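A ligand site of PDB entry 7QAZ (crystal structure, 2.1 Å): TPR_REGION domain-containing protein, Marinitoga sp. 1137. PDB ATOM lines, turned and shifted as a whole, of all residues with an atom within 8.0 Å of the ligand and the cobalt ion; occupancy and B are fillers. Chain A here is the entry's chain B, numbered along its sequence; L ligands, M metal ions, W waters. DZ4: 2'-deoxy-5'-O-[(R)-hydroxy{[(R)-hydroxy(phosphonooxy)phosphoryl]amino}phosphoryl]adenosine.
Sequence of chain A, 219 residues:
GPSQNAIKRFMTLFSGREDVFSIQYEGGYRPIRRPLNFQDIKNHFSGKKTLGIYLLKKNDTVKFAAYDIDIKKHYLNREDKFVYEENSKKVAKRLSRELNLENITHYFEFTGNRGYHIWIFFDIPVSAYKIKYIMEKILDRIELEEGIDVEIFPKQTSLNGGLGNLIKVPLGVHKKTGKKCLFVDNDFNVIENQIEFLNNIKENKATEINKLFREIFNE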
ATOM      1  N   GLU A  86     -19.043  33.822  -6.359  1.00  0.00           N
ATOM      2  CA  GLU A  86     -19.507  32.682  -5.565  1.00  0.00           C
ATOM      3  C   GLU A  86     -20.434  33.131  -4.458  1.00  0.00           C
ATOM      4  O   GLU A  86     -21.536  32.597  -4.301  1.00  0.00           O
ATOM      5  CB  GLU A  86     -18.334  31.904  -4.972  1.00  0.00           C
ATOM      6  CG  GLU A  86     -17.119  31.695  -5.871  1.00  0.00           C
ATOM      7  CD  GLU A  86     -16.241  30.579  -5.348  1.00  0.00           C
ATOM      8  OE1 GLU A  86     -15.960  30.638  -4.129  1.00  0.00           O
ATOM      9  OE2 GLU A  86     -15.782  29.705  -6.134  1.00  0.00           O
ATOM     10  N   LYS A  89     -23.928  33.848  -5.317  1.00  0.00           N
ATOM     11  CA  LYS A  89     -24.743  32.647  -5.496  1.00  0.00           C
ATOM     12  C   LYS A  89     -25.076  31.988  -4.155  1.00  0.00           C
ATOM     13  O   LYS A  89     -26.164  31.416  -4.018  1.00  0.00           O
ATOM     14  CB  LYS A  89     -24.004  31.676  -6.407  1.00  0.00           C
ATOM     15  CG  LYS A  89     -23.746  32.275  -7.778  1.00  0.00           C
ATOM     16  CD  LYS A  89     -23.353  31.229  -8.794  1.00  0.00           C
ATOM     17  CE  LYS A  89     -22.084  31.628  -9.515  1.00  0.00           C
ATOM     18  NZ  LYS A  89     -21.934  30.825 -10.754  1.00  0.00           N
ATOM     19  N   LYS A  90     -24.162  32.071  -3.172  1.00  0.00           N
ATOM     20  CA  LYS A  90     -24.434  31.559  -1.837  1.00  0.00           C
ATOM     21  C   LYS A  90     -25.625  32.277  -1.197  1.00  0.00           C
ATOM     22  O   LYS A  90     -26.537  31.641  -0.655  1.00  0.00           O
ATOM     23  CB  LYS A  90     -23.187  31.708  -0.957  1.00  0.00           C
ATOM     24  CG  LYS A  90     -22.075  30.722  -1.295  1.00  0.00           C
ATOM     25  CD  LYS A  90     -20.813  31.074  -0.533  1.00  0.00           C
ATOM     26  CE  LYS A  90     -19.840  29.888  -0.486  1.00  0.00           C
ATOM     27  NZ  LYS A  90     -18.652  30.188   0.358  1.00  0.00           N
ATOM     28  N   LYS A  93     -28.868  31.284  -3.011  1.00  0.00           N
ATOM     29  CA  LYS A  93     -29.345  29.960  -2.631  1.00  0.00           C
ATOM     30  C   LYS A  93     -30.009  29.993  -1.255  1.00  0.00           C
ATOM     31  O   LYS A  93     -31.018  29.306  -1.024  1.00  0.00           O
ATOM     32  CB  LYS A  93     -28.192  28.943  -2.633  1.00  0.00           C
ATOM     33  CG  LYS A  93     -27.680  28.578  -4.013  1.00  0.00           C
ATOM     34  CD  LYS A  93     -28.816  28.475  -5.031  1.00  0.00           C
ATOM     35  CE  LYS A  93     -29.382  27.075  -5.100  1.00  0.00           C
ATOM     36  NZ  LYS A  93     -28.295  26.071  -5.249  1.00  0.00           N
ATOM     37  N   ARG A  94     -29.459  30.753  -0.312  1.00  0.00           N
ATOM     38  CA  ARG A  94     -30.079  30.833   1.005  1.00  0.00           C
ATOM     39  C   ARG A  94     -31.477  31.421   0.916  1.00  0.00           C
ATOM     40  O   ARG A  94     -32.438  30.855   1.449  1.00  0.00           O
ATOM     41  CB  ARG A  94     -29.186  31.642   1.956  1.00  0.00           C
ATOM     42  CG  ARG A  94     -27.949  30.905   2.348  1.00  0.00           C
ATOM     43  CD  ARG A  94     -26.829  31.841   2.749  1.00  0.00           C
ATOM     44  NE  ARG A  94     -25.580  31.099   2.925  1.00  0.00           N
ATOM     45  CZ  ARG A  94     -24.392  31.665   3.082  1.00  0.00           C
ATOM     46  NH1 ARG A  94     -24.253  32.983   3.151  1.00  0.00           N
ATOM     47  NH2 ARG A  94     -23.326  30.884   3.196  1.00  0.00           N
ATOM     48  N   SER A  96     -33.483  31.527  -1.627  1.00  0.00           N
ATOM     49  CA  SER A  96     -34.336  30.590  -2.363  1.00  0.00           C
ATOM     50  C   SER A  96     -34.798  29.431  -1.468  1.00  0.00           C
ATOM     51  O   SER A  96     -35.953  28.990  -1.559  1.00  0.00           O
ATOM     52  CB  SER A  96     -33.580  30.077  -3.582  1.00  0.00           C
ATOM     53  OG  SER A  96     -34.063  28.812  -4.025  1.00  0.00           O
ATOM     54  N   ARG A  97     -33.893  28.923  -0.628  1.00  0.00           N
ATOM     55  CA  ARG A  97     -34.281  27.864   0.313  1.00  0.00           C
ATOM     56  C   ARG A  97     -35.395  28.330   1.244  1.00  0.00           C
ATOM     57  O   ARG A  97     -36.374  27.594   1.479  1.00  0.00           O
ATOM     58  CB  ARG A  97     -33.059  27.401   1.117  1.00  0.00           C
ATOM     59  CG  ARG A  97     -32.154  26.417   0.392  1.00  0.00           C
ATOM     60  CD  ARG A  97     -31.321  25.554   1.363  1.00  0.00           C
ATOM     61  NE  ARG A  97     -30.163  26.234   1.964  1.00  0.00           N
ATOM     62  CZ  ARG A  97     -29.010  26.459   1.328  1.00  0.00           C
ATOM     63  NH1 ARG A  97     -28.854  26.194   0.040  1.00  0.00           N
ATOM     64  NH2 ARG A  97     -27.984  26.970   2.012  1.00  0.00           N
ATOM     65  N   ASN A 100     -38.645  28.557  -0.828  1.00  0.00           N
ATOM     66  CA  ASN A 100     -39.229  27.234  -1.030  1.00  0.00           C
ATOM     67  C   ASN A 100     -39.898  26.733   0.244  1.00  0.00           C
ATOM     68  O   ASN A 100     -40.954  26.094   0.203  1.00  0.00           O
ATOM     69  CB  ASN A 100     -38.156  26.259  -1.501  1.00  0.00           C
ATOM     70  CG  ASN A 100     -37.778  26.444  -2.973  1.00  0.00           C
ATOM     71  OD1 ASN A 100     -38.589  26.917  -3.784  1.00  0.00           O
ATOM     72  ND2 ASN A 100     -36.554  26.078  -3.316  1.00  0.00           N
ATOM     73  N   PHE A 108     -34.684  32.261 -10.984  1.00  0.00           N
ATOM     74  CA  PHE A 108     -33.394  32.947 -10.984  1.00  0.00           C
ATOM     75  C   PHE A 108     -33.166  33.588 -12.338  1.00  0.00           C
ATOM     76  O   PHE A 108     -33.507  33.024 -13.372  1.00  0.00           O
ATOM     77  CB  PHE A 108     -32.221  31.979 -10.737  1.00  0.00           C
ATOM     78  CG  PHE A 108     -32.151  31.386  -9.358  1.00  0.00           C
ATOM     79  CD1 PHE A 108     -32.926  31.861  -8.329  1.00  0.00           C
ATOM     80  CD2 PHE A 108     -31.292  30.333  -9.107  1.00  0.00           C
ATOM     81  CE1 PHE A 108     -32.848  31.294  -7.063  1.00  0.00           C
ATOM     82  CE2 PHE A 108     -31.217  29.772  -7.848  1.00  0.00           C
ATOM     83  CZ  PHE A 108     -31.998  30.258  -6.834  1.00  0.00           C
ATOM     84  N   ASP A 185     -30.870  28.143 -14.065  1.00  0.00           N
ATOM     85  CA  ASP A 185     -31.532  27.124 -13.263  1.00  0.00           C
ATOM     86  C   ASP A 185     -31.080  27.285 -11.814  1.00  0.00           C
ATOM     87  O   ASP A 185     -30.364  28.220 -11.455  1.00  0.00           O
ATOM     88  CB  ASP A 185     -31.283  25.719 -13.801  1.00  0.00           C
ATOM     89  CG  ASP A 185     -29.793  25.343 -13.838  1.00  0.00           C
ATOM     90  OD1 ASP A 185     -28.961  25.987 -13.152  1.00  0.00           O
ATOM     91  OD2 ASP A 185     -29.460  24.353 -14.545  1.00  0.00           O
ATOM     92  N   ASN A 186     -31.491  26.337 -10.953  1.00  0.00           N
ATOM     93  CA  ASN A 186     -31.138  26.423  -9.547  1.00  0.00           C
ATOM     94  C   ASN A 186     -29.641  26.326  -9.305  1.00  0.00           C
ATOM     95  O   ASN A 186     -29.165  26.720  -8.239  1.00  0.00           O
ATOM     96  CB  ASN A 186     -31.866  25.322  -8.780  1.00  0.00           C
ATOM     97  CG  ASN A 186     -31.656  25.429  -7.292  1.00  0.00           C
ATOM     98  OD1 ASN A 186     -32.284  26.268  -6.623  1.00  0.00           O
ATOM     99  ND2 ASN A 186     -30.774  24.593  -6.761  1.00  0.00           N
ATOM    100  N   ASP A 187     -28.872  25.861 -10.299  1.00  0.00           N
ATOM    101  CA  ASP A 187     -27.419  25.851 -10.223  1.00  0.00           C
ATOM    102  C   ASP A 187     -26.788  27.072 -10.891  1.00  0.00           C
ATOM    103  O   ASP A 187     -25.560  27.103 -11.036  1.00  0.00           O
ATOM    104  CB  ASP A 187     -26.868  24.589 -10.861  1.00  0.00           C
ATOM    105  CG  ASP A 187     -27.145  23.361 -10.047  1.00  0.00           C
ATOM    106  OD1 ASP A 187     -27.018  23.458  -8.807  1.00  0.00           O
ATOM    107  OD2 ASP A 187     -27.497  22.331 -10.627  1.00  0.00           O
ATOM    108  N   PHE A 188     -27.604  28.029 -11.320  1.00  0.00           N
ATOM    109  CA  PHE A 188     -27.177  29.261 -11.994  1.00  0.00           C
ATOM    110  C   PHE A 188     -26.660  29.008 -13.411  1.00  0.00           C
ATOM    111  O   PHE A 188     -25.969  29.861 -13.982  1.00  0.00           O
ATOM    112  CB  PHE A 188     -26.143  30.019 -11.171  1.00  0.00           C
ATOM    113  CG  PHE A 188     -26.617  30.360  -9.797  1.00  0.00           C
ATOM    114  CD1 PHE A 188     -27.345  31.523  -9.566  1.00  0.00           C
ATOM    115  CD2 PHE A 188     -26.382  29.509  -8.734  1.00  0.00           C
ATOM    116  CE1 PHE A 188     -27.818  31.837  -8.302  1.00  0.00           C
ATOM    117  CE2 PHE A 188     -26.846  29.813  -7.468  1.00  0.00           C
ATOM    118  CZ  PHE A 188     -27.563  30.983  -7.248  1.00  0.00           C
ATOM    119  N   ASN A 189     -26.983  27.859 -13.998  1.00  0.00           N
ATOM    120  CA  ASN A 189     -26.632  27.579 -15.385  1.00  0.00           C
ATOM    121  C   ASN A 189     -27.723  28.096 -16.329  1.00  0.00           C
ATOM    122  O   ASN A 189     -28.917  27.945 -16.064  1.00  0.00           O
ATOM    123  CB  ASN A 189     -26.420  26.074 -15.580  1.00  0.00           C
ATOM    124  CG  ASN A 189     -25.204  25.558 -14.825  1.00  0.00           C
ATOM    125  OD1 ASN A 189     -24.192  26.244 -14.734  1.00  0.00           O
ATOM    126  ND2 ASN A 189     -25.319  24.356 -14.261  1.00  0.00           N
HETATM  127  N1  DZ4 L   1     -17.075  18.141  -2.215  1.00  0.00           N
HETATM  128  C2  DZ4 L   1     -18.142  17.984  -3.065  1.00  0.00           C
HETATM  129  N3  DZ4 L   1     -18.486  18.992  -3.921  1.00  0.00           N
HETATM  130  C4  DZ4 L   1     -17.760  20.146  -3.949  1.00  0.00           C
HETATM  131  C5  DZ4 L   1     -16.714  20.301  -3.119  1.00  0.00           C
HETATM  132  C6  DZ4 L   1     -16.370  19.286  -2.241  1.00  0.00           C
HETATM  133  N6  DZ4 L   1     -15.310  19.119  -1.250  1.00  0.00           N
HETATM  134  N7  DZ4 L   1     -16.152  21.497  -3.338  1.00  0.00           N
HETATM  135  C8  DZ4 L   1     -16.860  22.102  -4.299  1.00  0.00           C
HETATM  136  N9  DZ4 L   1     -17.841  21.281  -4.681  1.00  0.00           N
HETATM  137  PA  DZ4 L   1     -23.854  23.210  -4.554  1.00  0.00           P
HETATM  138  PB  DZ4 L   1     -25.668  20.969  -3.768  1.00  0.00           P
HETATM  139  PG  DZ4 L   1     -28.099  22.621  -3.466  1.00  0.00           P
HETATM  140  C1' DZ4 L   1     -18.825  21.575  -5.713  1.00  0.00           C
HETATM  141  O1A DZ4 L   1     -24.479  23.154  -5.938  1.00  0.00           O
HETATM  142  O1B DZ4 L   1     -25.146  19.928  -2.796  1.00  0.00           O
HETATM  143  O1G DZ4 L   1     -29.587  22.378  -3.571  1.00  0.00           O
HETATM  144  C2' DZ4 L   1     -19.186  20.320  -6.687  1.00  0.00           C
HETATM  145  O2A DZ4 L   1     -23.643  24.657  -4.147  1.00  0.00           O
HETATM  146  O2B DZ4 L   1     -25.413  20.515  -5.180  1.00  0.00           O
HETATM  147  O2G DZ4 L   1     -27.778  23.316  -2.160  1.00  0.00           O
HETATM  148  C3' DZ4 L   1     -20.432  20.052  -6.449  1.00  0.00           C
HETATM  149  O3' DZ4 L   1     -21.152  19.427  -7.617  1.00  0.00           O
HETATM  150  N3A DZ4 L   1     -24.870  22.437  -3.425  1.00  0.00           N
HETATM  151  O3B DZ4 L   1     -27.298  21.167  -3.549  1.00  0.00           O
HETATM  152  O3G DZ4 L   1     -27.666  23.503  -4.617  1.00  0.00           O
HETATM  153  C4' DZ4 L   1     -21.007  21.441  -6.123  1.00  0.00           C
HETATM  154  O4' DZ4 L   1     -19.945  21.944  -5.161  1.00  0.00           O
HETATM  155  C5' DZ4 L   1     -22.267  21.348  -5.493  1.00  0.00           C
HETATM  156  O5' DZ4 L   1     -22.403  22.434  -4.622  1.00  0.00           O
HETATM  157 CO    CO M   1     -27.013  22.401  -6.848  1.00  0.00          CO
HETATM  158  O   HOH W   1     -27.369  21.525   0.443  1.00  0.00           O
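The side-chain amino group (NZ) of Lys 93 lies close to an oxygen (O3G) of the ligand (2.7 Å). An oxygen (O2G) of the ligand lies within salt-bridge range of the guanidinium group (NH1) of Arg 97 (3.8 Å).
The backbone NH (N) of Asp 187 sits at hydrogen-bond distance from the side-chain carboxylate (OD1) of Asp 185, 2.9 Å away. NZ of Lys 93 lies close to O of Asn 186, 3.2 Å away.
Residues that only touch the ligand: Asn 186. Within 4 Å of the ligand: Lys 93, Arg 97, Asn 186 and Asp 187. The nearest printed residue that does not touch the ligand is Lys 90 (6.9 Å).
Within 4 Å of the cobalt ion: Asp 187.
The cobalt ion is bound by OD1 of Asp 187 (2.2 Å) and O3G of the ligand (2.6 Å). Slightly farther from the cobalt ion lies an oxygen (O1A) of the ligand (2.8 Å).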
